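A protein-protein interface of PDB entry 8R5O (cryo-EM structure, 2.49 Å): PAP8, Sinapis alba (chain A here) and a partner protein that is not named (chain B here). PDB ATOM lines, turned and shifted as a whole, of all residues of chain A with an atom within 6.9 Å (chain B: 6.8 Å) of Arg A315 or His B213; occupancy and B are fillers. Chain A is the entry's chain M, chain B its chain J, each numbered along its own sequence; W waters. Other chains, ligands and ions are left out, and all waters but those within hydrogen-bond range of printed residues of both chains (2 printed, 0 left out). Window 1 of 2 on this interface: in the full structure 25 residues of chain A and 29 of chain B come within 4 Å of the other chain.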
ATOM      1  N   GLU A 310      18.902  -0.739  32.500  1.00  0.00           N
ATOM      2  CA  GLU A 310      19.921   0.303  32.452  1.00  0.00           C
ATOM      3  C   GLU A 310      20.245   0.700  31.018  1.00  0.00           C
ATOM      4  O   GLU A 310      20.423   1.887  30.724  1.00  0.00           O
ATOM      5  CB  GLU A 310      21.180  -0.159  33.183  1.00  0.00           C
ATOM      6  CG  GLU A 310      20.968  -0.383  34.667  1.00  0.00           C
ATOM      7  CD  GLU A 310      22.201  -0.916  35.365  1.00  0.00           C
ATOM      8  OE1 GLU A 310      23.187  -1.249  34.675  1.00  0.00           O
ATOM      9  OE2 GLU A 310      22.185  -1.002  36.610  1.00  0.00           O
ATOM     10  N   TRP A 311      20.334  -0.276  30.113  1.00  0.00           N
ATOM     11  CA  TRP A 311      20.651   0.037  28.724  1.00  0.00           C
ATOM     12  C   TRP A 311      19.560   0.889  28.091  1.00  0.00           C
ATOM     13  O   TRP A 311      19.853   1.845  27.367  1.00  0.00           O
ATOM     14  CB  TRP A 311      20.860  -1.249  27.928  1.00  0.00           C
ATOM     15  CG  TRP A 311      21.774  -1.082  26.754  1.00  0.00           C
ATOM     16  CD1 TRP A 311      23.115  -1.320  26.722  1.00  0.00           C
ATOM     17  CD2 TRP A 311      21.414  -0.642  25.439  1.00  0.00           C
ATOM     18  NE1 TRP A 311      23.615  -1.056  25.473  1.00  0.00           N
ATOM     19  CE2 TRP A 311      22.591  -0.638  24.666  1.00  0.00           C
ATOM     20  CE3 TRP A 311      20.213  -0.250  24.843  1.00  0.00           C
ATOM     21  CZ2 TRP A 311      22.602  -0.258  23.328  1.00  0.00           C
ATOM     22  CZ3 TRP A 311      20.227   0.126  23.515  1.00  0.00           C
ATOM     23  CH2 TRP A 311      21.413   0.119  22.771  1.00  0.00           C
ATOM     24  N   THR A 312      18.296   0.559  28.358  1.00  0.00           N
ATOM     25  CA  THR A 312      17.190   1.327  27.797  1.00  0.00           C
ATOM     26  C   THR A 312      17.194   2.763  28.308  1.00  0.00           C
ATOM     27  O   THR A 312      16.957   3.703  27.542  1.00  0.00           O
ATOM     28  CB  THR A 312      15.862   0.646  28.127  1.00  0.00           C
ATOM     29  OG1 THR A 312      15.827  -0.650  27.517  1.00  0.00           O
ATOM     30  CG2 THR A 312      14.692   1.469  27.617  1.00  0.00           C
ATOM     31  N   LYS A 313      17.467   2.953  29.600  1.00  0.00           N
ATOM     32  CA  LYS A 313      17.424   4.292  30.175  1.00  0.00           C
ATOM     33  C   LYS A 313      18.604   5.137  29.709  1.00  0.00           C
ATOM     34  O   LYS A 313      18.436   6.307  29.345  1.00  0.00           O
ATOM     35  CB  LYS A 313      17.396   4.210  31.699  1.00  0.00           C
ATOM     36  CG  LYS A 313      17.146   5.545  32.370  1.00  0.00           C
ATOM     37  CD  LYS A 313      17.358   5.470  33.868  1.00  0.00           C
ATOM     38  CE  LYS A 313      17.005   6.791  34.530  1.00  0.00           C
ATOM     39  NZ  LYS A 313      17.710   7.938  33.897  1.00  0.00           N
ATOM     40  N   THR A 314      19.811   4.566  29.717  1.00  0.00           N
ATOM     41  CA  THR A 314      20.984   5.335  29.311  1.00  0.00           C
ATOM     42  C   THR A 314      20.984   5.617  27.816  1.00  0.00           C
ATOM     43  O   THR A 314      21.523   6.640  27.382  1.00  0.00           O
ATOM     44  CB  THR A 314      22.266   4.605  29.711  1.00  0.00           C
ATOM     45  OG1 THR A 314      22.257   3.283  29.162  1.00  0.00           O
ATOM     46  CG2 THR A 314      22.387   4.524  31.224  1.00  0.00           C
ATOM     47  N   ARG A 315      20.398   4.725  27.014  1.00  0.00           N
ATOM     48  CA  ARG A 315      20.305   4.969  25.579  1.00  0.00           C
ATOM     49  C   ARG A 315      19.436   6.184  25.283  1.00  0.00           C
ATOM     50  O   ARG A 315      19.769   6.998  24.413  1.00  0.00           O
ATOM     51  CB  ARG A 315      19.759   3.728  24.872  1.00  0.00           C
ATOM     52  CG  ARG A 315      19.475   3.908  23.391  1.00  0.00           C
ATOM     53  CD  ARG A 315      20.742   4.167  22.598  1.00  0.00           C
ATOM     54  NE  ARG A 315      20.479   4.258  21.166  1.00  0.00           N
ATOM     55  CZ  ARG A 315      20.056   5.353  20.552  1.00  0.00           C
ATOM     56  NH1 ARG A 315      19.825   6.473  21.215  1.00  0.00           N
ATOM     57  NH2 ARG A 315      19.855   5.323  19.237  1.00  0.00           N
ATOM     58  N   GLU A 316      18.319   6.327  25.998  1.00  0.00           N
ATOM     59  CA  GLU A 316      17.447   7.476  25.783  1.00  0.00           C
ATOM     60  C   GLU A 316      18.072   8.758  26.323  1.00  0.00           C
ATOM     61  O   GLU A 316      17.955   9.820  25.702  1.00  0.00           O
ATOM     62  CB  GLU A 316      16.084   7.225  26.428  1.00  0.00           C
ATOM     63  CG  GLU A 316      15.154   8.423  26.386  1.00  0.00           C
ATOM     64  CD  GLU A 316      14.959   8.958  24.981  1.00  0.00           C
ATOM     65  OE1 GLU A 316      14.577   8.172  24.089  1.00  0.00           O
ATOM     66  OE2 GLU A 316      15.202  10.164  24.767  1.00  0.00           O
ATOM     67  N   ASP A 317      18.737   8.678  27.478  1.00  0.00           N
ATOM     68  CA  ASP A 317      19.364   9.863  28.058  1.00  0.00           C
ATOM     69  C   ASP A 317      20.514  10.370  27.195  1.00  0.00           C
ATOM     70  O   ASP A 317      20.693  11.584  27.045  1.00  0.00           O
ATOM     71  CB  ASP A 317      19.852   9.560  29.474  1.00  0.00           C
ATOM     72  CG  ASP A 317      18.717   9.465  30.472  1.00  0.00           C
ATOM     73  OD1 ASP A 317      17.562   9.738  30.090  1.00  0.00           O
ATOM     74  OD2 ASP A 317      18.980   9.116  31.642  1.00  0.00           O
ATOM     75  N   MET A 318      21.311   9.459  26.633  1.00  0.00           N
ATOM     76  CA  MET A 318      22.425   9.875  25.787  1.00  0.00           C
ATOM     77  C   MET A 318      21.934  10.594  24.537  1.00  0.00           C
ATOM     78  O   MET A 318      22.483  11.635  24.157  1.00  0.00           O
ATOM     79  CB  MET A 318      23.275   8.664  25.408  1.00  0.00           C
ATOM     80  CG  MET A 318      24.385   8.968  24.417  1.00  0.00           C
ATOM     81  SD  MET A 318      25.589  10.150  25.051  1.00  0.00           S
ATOM     82  CE  MET A 318      26.305   9.208  26.390  1.00  0.00           C
ATOM     83  N   GLU A 319      20.899  10.060  23.887  1.00  0.00           N
ATOM     84  CA  GLU A 319      20.378  10.701  22.683  1.00  0.00           C
ATOM     85  C   GLU A 319      19.786  12.067  22.999  1.00  0.00           C
ATOM     86  O   GLU A 319      19.918  13.006  22.207  1.00  0.00           O
ATOM     87  CB  GLU A 319      19.341   9.804  22.012  1.00  0.00           C
ATOM     88  CG  GLU A 319      18.795  10.372  20.715  1.00  0.00           C
ATOM     89  CD  GLU A 319      17.855   9.424  20.006  1.00  0.00           C
ATOM     90  OE1 GLU A 319      17.949   8.203  20.243  1.00  0.00           O
ATOM     91  OE2 GLU A 319      17.021   9.902  19.210  1.00  0.00           O
ATOM     92  N   LYS A 320      19.130  12.194  24.154  1.00  0.00           N
ATOM     93  CA  LYS A 320      18.624  13.491  24.588  1.00  0.00           C
ATOM     94  C   LYS A 320      19.761  14.482  24.802  1.00  0.00           C
ATOM     95  O   LYS A 320      19.640  15.663  24.457  1.00  0.00           O
ATOM     96  CB  LYS A 320      17.804  13.312  25.866  1.00  0.00           C
ATOM     97  CG  LYS A 320      17.366  14.592  26.542  1.00  0.00           C
ATOM     98  CD  LYS A 320      16.647  14.268  27.840  1.00  0.00           C
ATOM     99  CE  LYS A 320      16.343  15.517  28.646  1.00  0.00           C
ATOM    100  NZ  LYS A 320      15.612  15.186  29.900  1.00  0.00           N
ATOM    101  N   PHE A 328      23.609  16.587  14.787  1.00  0.00           N
ATOM    102  CA  PHE A 328      22.968  15.350  15.224  1.00  0.00           C
ATOM    103  C   PHE A 328      22.240  14.660  14.075  1.00  0.00           C
ATOM    104  O   PHE A 328      22.293  13.431  13.949  1.00  0.00           O
ATOM    105  CB  PHE A 328      22.005  15.655  16.373  1.00  0.00           C
ATOM    106  CG  PHE A 328      21.234  14.463  16.870  1.00  0.00           C
ATOM    107  CD1 PHE A 328      19.981  14.167  16.356  1.00  0.00           C
ATOM    108  CD2 PHE A 328      21.747  13.659  17.873  1.00  0.00           C
ATOM    109  CE1 PHE A 328      19.267  13.079  16.818  1.00  0.00           C
ATOM    110  CE2 PHE A 328      21.034  12.573  18.340  1.00  0.00           C
ATOM    111  CZ  PHE A 328      19.791  12.286  17.813  1.00  0.00           C
ATOM    112  N   SER A 331      24.396  12.290  11.848  1.00  0.00           N
ATOM    113  CA  SER A 331      25.298  11.449  12.618  1.00  0.00           C
ATOM    114  C   SER A 331      24.640  10.106  12.910  1.00  0.00           C
ATOM    115  O   SER A 331      23.416   9.971  12.893  1.00  0.00           O
ATOM    116  CB  SER A 331      25.715  12.132  13.926  1.00  0.00           C
ATOM    117  OG  SER A 331      24.584  12.474  14.701  1.00  0.00           O
ATOM    118  N   ASN A 332      25.479   9.110  13.178  1.00  0.00           N
ATOM    119  CA  ASN A 332      25.044   7.751  13.461  1.00  0.00           C
ATOM    120  C   ASN A 332      25.208   7.415  14.938  1.00  0.00           C
ATOM    121  O   ASN A 332      26.092   7.936  15.620  1.00  0.00           O
ATOM    122  CB  ASN A 332      25.840   6.736  12.637  1.00  0.00           C
ATOM    123  CG  ASN A 332      25.234   6.471  11.280  1.00  0.00           C
ATOM    124  OD1 ASN A 332      24.424   7.251  10.784  1.00  0.00           O
ATOM    125  ND2 ASN A 332      25.624   5.362  10.668  1.00  0.00           N
ATOM    126  N   TRP A 333      24.333   6.540  15.426  1.00  0.00           N
ATOM    127  CA  TRP A 333      24.613   5.795  16.642  1.00  0.00           C
ATOM    128  C   TRP A 333      25.543   4.631  16.319  1.00  0.00           C
ATOM    129  O   TRP A 333      25.473   4.040  15.241  1.00  0.00           O
ATOM    130  CB  TRP A 333      23.321   5.271  17.278  1.00  0.00           C
ATOM    131  CG  TRP A 333      23.568   4.224  18.330  1.00  0.00           C
ATOM    132  CD1 TRP A 333      23.659   2.877  18.140  1.00  0.00           C
ATOM    133  CD2 TRP A 333      23.781   4.445  19.730  1.00  0.00           C
ATOM    134  NE1 TRP A 333      23.911   2.245  19.330  1.00  0.00           N
ATOM    135  CE2 TRP A 333      23.989   3.185  20.323  1.00  0.00           C
ATOM    136  CE3 TRP A 333      23.813   5.583  20.538  1.00  0.00           C
ATOM    137  CZ2 TRP A 333      24.225   3.033  21.686  1.00  0.00           C
ATOM    138  CZ3 TRP A 333      24.048   5.430  21.890  1.00  0.00           C
ATOM    139  CH2 TRP A 333      24.250   4.165  22.451  1.00  0.00           C
ATOM    140  N   PHE A 334      26.423   4.308  17.260  1.00  0.00           N
ATOM    141  CA  PHE A 334      27.257   3.115  17.129  1.00  0.00           C
ATOM    142  C   PHE A 334      27.691   2.592  18.494  1.00  0.00           C
ATOM    143  O   PHE A 334      27.403   3.200  19.522  1.00  0.00           O
ATOM    144  CB  PHE A 334      28.484   3.398  16.253  1.00  0.00           C
ATOM    145  CG  PHE A 334      29.306   4.568  16.709  1.00  0.00           C
ATOM    146  CD1 PHE A 334      30.286   4.415  17.676  1.00  0.00           C
ATOM    147  CD2 PHE A 334      29.105   5.822  16.162  1.00  0.00           C
ATOM    148  CE1 PHE A 334      31.040   5.491  18.094  1.00  0.00           C
ATOM    149  CE2 PHE A 334      29.856   6.901  16.575  1.00  0.00           C
ATOM    150  CZ  PHE A 334      30.825   6.736  17.540  1.00  0.00           C
ATOM    151  N   GLY B 202      15.326  -3.721   8.852  1.00  0.00           N
ATOM    152  CA  GLY B 202      16.351  -2.696   8.773  1.00  0.00           C
ATOM    153  C   GLY B 202      16.342  -1.770   9.970  1.00  0.00           C
ATOM    154  O   GLY B 202      16.739  -2.160  11.067  1.00  0.00           O
ATOM    155  N   PHE B 203      15.892  -0.536   9.759  1.00  0.00           N
ATOM    156  CA  PHE B 203      15.766   0.405  10.861  1.00  0.00           C
ATOM    157  C   PHE B 203      14.715  -0.088  11.848  1.00  0.00           C
ATOM    158  O   PHE B 203      13.849  -0.900  11.510  1.00  0.00           O
ATOM    159  CB  PHE B 203      15.402   1.797  10.341  1.00  0.00           C
ATOM    160  CG  PHE B 203      15.731   2.910  11.298  1.00  0.00           C
ATOM    161  CD1 PHE B 203      14.797   3.352  12.218  1.00  0.00           C
ATOM    162  CD2 PHE B 203      16.974   3.518  11.271  1.00  0.00           C
ATOM    163  CE1 PHE B 203      15.096   4.373  13.094  1.00  0.00           C
ATOM    164  CE2 PHE B 203      17.279   4.540  12.144  1.00  0.00           C
ATOM    165  CZ  PHE B 203      16.339   4.969  13.056  1.00  0.00           C
ATOM    166  N   GLU B 204      14.832   0.387  13.089  1.00  0.00           N
ATOM    167  CA  GLU B 204      13.979   0.025  14.219  1.00  0.00           C
ATOM    168  C   GLU B 204      14.301  -1.378  14.721  1.00  0.00           C
ATOM    169  O   GLU B 204      13.806  -1.794  15.773  1.00  0.00           O
ATOM    170  CB  GLU B 204      12.492   0.145  13.863  1.00  0.00           C
ATOM    171  CG  GLU B 204      11.661   0.785  14.957  1.00  0.00           C
ATOM    172  CD  GLU B 204      12.111   2.198  15.274  1.00  0.00           C
ATOM    173  OE1 GLU B 204      12.449   2.942  14.329  1.00  0.00           O
ATOM    174  OE2 GLU B 204      12.137   2.564  16.468  1.00  0.00           O
ATOM    175  N   LEU B 205      15.138  -2.107  13.987  1.00  0.00           N
ATOM    176  CA  LEU B 205      15.790  -3.306  14.494  1.00  0.00           C
ATOM    177  C   LEU B 205      17.242  -3.046  14.865  1.00  0.00           C
ATOM    178  O   LEU B 205      17.710  -3.525  15.901  1.00  0.00           O
ATOM    179  CB  LEU B 205      15.720  -4.439  13.466  1.00  0.00           C
ATOM    180  CG  LEU B 205      16.478  -5.719  13.832  1.00  0.00           C
ATOM    181  CD1 LEU B 205      15.903  -6.349  15.092  1.00  0.00           C
ATOM    182  CD2 LEU B 205      16.473  -6.710  12.680  1.00  0.00           C
ATOM    183  N   ASP B 206      17.960  -2.288  14.033  1.00  0.00           N
ATOM    184  CA  ASP B 206      19.274  -1.794  14.425  1.00  0.00           C
ATOM    185  C   ASP B 206      19.168  -0.869  15.630  1.00  0.00           C
ATOM    186  O   ASP B 206      20.009  -0.916  16.536  1.00  0.00           O
ATOM    187  CB  ASP B 206      19.931  -1.067  13.252  1.00  0.00           C
ATOM    188  CG  ASP B 206      20.113  -1.956  12.040  1.00  0.00           C
ATOM    189  OD1 ASP B 206      19.919  -3.184  12.163  1.00  0.00           O
ATOM    190  OD2 ASP B 206      20.446  -1.425  10.960  1.00  0.00           O
ATOM    191  N   LYS B 207      18.142  -0.016  15.652  1.00  0.00           N
ATOM    192  CA  LYS B 207      17.943   0.893  16.776  1.00  0.00           C
ATOM    193  C   LYS B 207      17.638   0.131  18.060  1.00  0.00           C
ATOM    194  O   LYS B 207      18.109   0.509  19.138  1.00  0.00           O
ATOM    195  CB  LYS B 207      16.821   1.878  16.447  1.00  0.00           C
ATOM    196  CG  LYS B 207      16.598   2.969  17.480  1.00  0.00           C
ATOM    197  CD  LYS B 207      15.663   4.034  16.927  1.00  0.00           C
ATOM    198  CE  LYS B 207      15.490   5.194  17.889  1.00  0.00           C
ATOM    199  NZ  LYS B 207      14.769   4.789  19.123  1.00  0.00           N
ATOM    200  N   LYS B 208      16.845  -0.937  17.965  1.00  0.00           N
ATOM    201  CA  LYS B 208      16.519  -1.725  19.149  1.00  0.00           C
ATOM    202  C   LYS B 208      17.745  -2.447  19.697  1.00  0.00           C
ATOM    203  O   LYS B 208      17.938  -2.515  20.915  1.00  0.00           O
ATOM    204  CB  LYS B 208      15.413  -2.725  18.817  1.00  0.00           C
ATOM    205  CG  LYS B 208      15.042  -3.649  19.962  1.00  0.00           C
ATOM    206  CD  LYS B 208      14.016  -4.676  19.522  1.00  0.00           C
ATOM    207  CE  LYS B 208      13.686  -5.647  20.642  1.00  0.00           C
ATOM    208  NZ  LYS B 208      12.693  -6.670  20.211  1.00  0.00           N
ATOM    209  N   GLY B 210      21.003  -1.708  19.189  1.00  0.00           N
ATOM    210  CA  GLY B 210      22.196  -0.911  19.368  1.00  0.00           C
ATOM    211  C   GLY B 210      23.216  -1.024  18.259  1.00  0.00           C
ATOM    212  O   GLY B 210      24.337  -0.528  18.418  1.00  0.00           O
ATOM    213  N   ARG B 211      22.868  -1.667  17.147  1.00  0.00           N
ATOM    214  CA  ARG B 211      23.746  -1.730  15.994  1.00  0.00           C
ATOM    215  C   ARG B 211      23.845  -0.355  15.334  1.00  0.00           C
ATOM    216  O   ARG B 211      22.974   0.495  15.523  1.00  0.00           O
ATOM    217  CB  ARG B 211      23.229  -2.766  15.001  1.00  0.00           C
ATOM    218  CG  ARG B 211      23.888  -4.126  15.133  1.00  0.00           C
ATOM    219  CD  ARG B 211      22.912  -5.251  14.840  1.00  0.00           C
ATOM    220  NE  ARG B 211      22.157  -5.030  13.615  1.00  0.00           N
ATOM    221  CZ  ARG B 211      21.280  -5.888  13.114  1.00  0.00           C
ATOM    222  NH1 ARG B 211      21.038  -7.050  13.700  1.00  0.00           N
ATOM    223  NH2 ARG B 211      20.628  -5.574  11.998  1.00  0.00           N
ATOM    224  N   PRO B 212      24.912  -0.107  14.571  1.00  0.00           N
ATOM    225  CA  PRO B 212      25.064   1.206  13.934  1.00  0.00           C
ATOM    226  C   PRO B 212      23.880   1.540  13.038  1.00  0.00           C
ATOM    227  O   PRO B 212      23.413   0.711  12.254  1.00  0.00           O
ATOM    228  CB  PRO B 212      26.358   1.060  13.128  1.00  0.00           C
ATOM    229  CG  PRO B 212      27.117   0.000  13.835  1.00  0.00           C
ATOM    230  CD  PRO B 212      26.088  -0.964  14.343  1.00  0.00           C
ATOM    231  N   HIS B 213      23.399   2.771  13.167  1.00  0.00           N
ATOM    232  CA  HIS B 213      22.224   3.238  12.448  1.00  0.00           C
ATOM    233  C   HIS B 213      22.153   4.757  12.529  1.00  0.00           C
ATOM    234  O   HIS B 213      22.695   5.349  13.471  1.00  0.00           O
ATOM    235  CB  HIS B 213      20.950   2.611  13.023  1.00  0.00           C
ATOM    236  CG  HIS B 213      20.558   3.155  14.362  1.00  0.00           C
ATOM    237  ND1 HIS B 213      19.868   4.338  14.513  1.00  0.00           N
ATOM    238  CD2 HIS B 213      20.758   2.676  15.612  1.00  0.00           C
ATOM    239  CE1 HIS B 213      19.662   4.565  15.797  1.00  0.00           C
ATOM    240  NE2 HIS B 213      20.192   3.571  16.484  1.00  0.00           N
ATOM    241  N   PRO B 214      21.512   5.422  11.571  1.00  0.00           N
ATOM    242  CA  PRO B 214      21.328   6.872  11.689  1.00  0.00           C
ATOM    243  C   PRO B 214      20.509   7.213  12.923  1.00  0.00           C
ATOM    244  O   PRO B 214      19.593   6.482  13.304  1.00  0.00           O
ATOM    245  CB  PRO B 214      20.586   7.243  10.400  1.00  0.00           C
ATOM    246  CG  PRO B 214      20.853   6.125   9.465  1.00  0.00           C
ATOM    247  CD  PRO B 214      20.965   4.899  10.308  1.00  0.00           C
ATOM    248  N   PHE B 215      20.852   8.336  13.555  1.00  0.00           N
ATOM    249  CA  PHE B 215      20.071   8.789  14.701  1.00  0.00           C
ATOM    250  C   PHE B 215      18.640   9.116  14.304  1.00  0.00           C
ATOM    251  O   PHE B 215      17.714   8.913  15.096  1.00  0.00           O
ATOM    252  CB  PHE B 215      20.735  10.003  15.346  1.00  0.00           C
ATOM    253  CG  PHE B 215      21.667   9.658  16.468  1.00  0.00           C
ATOM    254  CD1 PHE B 215      21.192   9.039  17.610  1.00  0.00           C
ATOM    255  CD2 PHE B 215      23.013   9.966  16.389  1.00  0.00           C
ATOM    256  CE1 PHE B 215      22.043   8.724  18.648  1.00  0.00           C
ATOM    257  CE2 PHE B 215      23.868   9.655  17.423  1.00  0.00           C
ATOM    258  CZ  PHE B 215      23.383   9.034  18.553  1.00  0.00           C
ATOM    259  N   ILE B 216      18.438   9.613  13.088  1.00  0.00           N
ATOM    260  CA  ILE B 216      17.119   9.940  12.565  1.00  0.00           C
ATOM    261  C   ILE B 216      16.833   9.012  11.394  1.00  0.00           C
ATOM    262  O   ILE B 216      17.670   8.864  10.496  1.00  0.00           O
ATOM    263  CB  ILE B 216      17.031  11.415  12.136  1.00  0.00           C
ATOM    264  CG1 ILE B 216      17.203  12.325  13.354  1.00  0.00           C
ATOM    265  CG2 ILE B 216      15.716  11.694  11.429  1.00  0.00           C
ATOM    266  CD1 ILE B 216      17.167  13.790  13.028  1.00  0.00           C
ATOM    267  N   ASP B 217      15.664   8.386  11.413  1.00  0.00           N
ATOM    268  CA  ASP B 217      15.263   7.474  10.351  1.00  0.00           C
ATOM    269  C   ASP B 217      15.194   8.225   9.026  1.00  0.00           C
ATOM    270  O   ASP B 217      14.484   9.237   8.935  1.00  0.00           O
ATOM    271  CB  ASP B 217      13.908   6.853  10.690  1.00  0.00           C
ATOM    272  CG  ASP B 217      13.610   5.600   9.886  1.00  0.00           C
ATOM    273  OD1 ASP B 217      14.193   5.415   8.800  1.00  0.00           O
ATOM    274  OD2 ASP B 217      12.776   4.795  10.347  1.00  0.00           O
ATOM    275  N   LYS B 270      30.034   1.917  11.801  1.00  0.00           N
ATOM    276  CA  LYS B 270      29.638   2.637  10.598  1.00  0.00           C
ATOM    277  C   LYS B 270      29.259   4.063  10.964  1.00  0.00           C
ATOM    278  O   LYS B 270      28.552   4.294  11.948  1.00  0.00           O
ATOM    279  CB  LYS B 270      28.463   1.954   9.889  1.00  0.00           C
ATOM    280  CG  LYS B 270      28.822   0.649   9.207  1.00  0.00           C
ATOM    281  CD  LYS B 270      27.698   0.171   8.300  1.00  0.00           C
ATOM    282  CE  LYS B 270      28.088  -1.105   7.572  1.00  0.00           C
ATOM    283  NZ  LYS B 270      27.031  -1.554   6.623  1.00  0.00           N
ATOM    284  N   TYR B 272      27.841   8.062   9.624  1.00  0.00           N
ATOM    285  CA  TYR B 272      26.896   8.651   8.683  1.00  0.00           C
ATOM    286  C   TYR B 272      27.593   9.077   7.396  1.00  0.00           C
ATOM    287  O   TYR B 272      27.055   8.888   6.299  1.00  0.00           O
ATOM    288  CB  TYR B 272      26.186   9.837   9.333  1.00  0.00           C
ATOM    289  CG  TYR B 272      25.003  10.353   8.547  1.00  0.00           C
ATOM    290  CD1 TYR B 272      25.167  11.305   7.549  1.00  0.00           C
ATOM    291  CD2 TYR B 272      23.722   9.889   8.805  1.00  0.00           C
ATOM    292  CE1 TYR B 272      24.087  11.776   6.831  1.00  0.00           C
ATOM    293  CE2 TYR B 272      22.637  10.356   8.092  1.00  0.00           C
ATOM    294  CZ  TYR B 272      22.826  11.298   7.106  1.00  0.00           C
ATOM    295  OH  TYR B 272      21.745  11.764   6.396  1.00  0.00           O
HETATM  296  O   HOH W   1      20.902  10.921  11.511  1.00  0.00           O
HETATM  297  O   HOH W   2      20.673   1.973  19.159  1.00  0.00           O
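The side-chain amide nitrogen (ND2) of Asn A332 lies within hydrogen-bond range of the backbone carbonyl oxygen (O) of Lys B270, at 3.4 Å. N of Phe B215 sits at hydrogen-bond distance from O of Ser A331 (3.1 Å). The guanidinium group (NH2) of Arg A315 lies within hydrogen-bond range of a ring nitrogen (NE2) of His B213 (3.3 Å). The backbone carbonyl oxygen of His B213 is in hydrogen-bond range of the backbone NH of Trp A333, at 2.8 Å. The indole nitrogen of Trp A333 is in hydrogen-bond range of the backbone carbonyl oxygen of Gly B210 (3.0 Å).
The backbone carbonyl oxygen (O) of Phe A328 is in hydrogen-bond range of the side-chain hydroxyl (OG) of Ser A331 (2.6 Å). The side-chain hydroxyl (OG1) of Thr A314 is in hydrogen-bond range of the backbone carbonyl oxygen (O) of Trp A311, at 3.3 Å. The guanidinium group (NH1) of Arg A315 is in salt-bridge range of the side-chain carboxylate (OE1) of Glu A319 (2.7 Å). The guanidinium group (NH2) of Arg B211 lies within salt-bridge range of the side-chain carboxylate (OD1) of Asp B206, 2.5 Å away.
Gly B210 touches Trp A311 (CA to CH2, 3.6 Å). Phe A328 touches Phe B215. O of Ser A331 touches CA of Pro B214, 3.9 Å away. Ser A331 touches Tyr B272 (CA to CB, 3.8 Å). His B213 touches Asn A332 (O to CA, 3.4 Å). Asn A332 touches Pro B214. Phe B215 touches Asn A332. Tyr B272 touches Asn A332 (CD2 to OD1, 3.4 Å). O of Arg B211 touches CD1 of Trp A333 (3.6 Å). Phe B215 touches Trp A333.
Of the printed residues of chain B, Arg A315 touches His B213. Glu A319 touches none of the printed residues of chain B. Printed residues of chain B within 4 Å of Ser A331: Pro B214, Phe B215 and Tyr B272. Lys B207 touches none of the printed residues of chain A. Printed residues of chain A within 4 Å of Pro B214: Ser A331 and Asn A332. Printed residues of chain A within 4 Å of Lys B270: Asn A332 (3.4 Å). The nearest residue of chain B that does not touch Arg A315 is Phe B215 (4.1 Å). The nearest residue of chain A that does not touch His B213 is Ser A331 (4.7 Å). The nearest printed residue of chain A that does not touch Pro B212 is Phe A334 (4.3 Å).
Printed residues of chain A that touch a printed residue of chain B: Trp A311, Arg A315, Phe A328, Ser A331, Asn A332 and Trp A333. Hydrophobic or aromatic side chains of chain B within 4 Å of the printed part of chain A: Pro B212, His B213, Pro B214, Phe B215 and Tyr B272.
Water W2 lies within hydrogen-bond range of O of Lys B207 (3.0 Å), NE of Arg A315 (3.0 Å), NE2 of His B213 (3.2 Å) and NE1 of Trp A333 (3.3 Å). Water W1 lies within hydrogen-bond range of the backbone carbonyl oxygen of Ser A331, the backbone NH of Ile B216 and the backbone NH of Phe B215.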
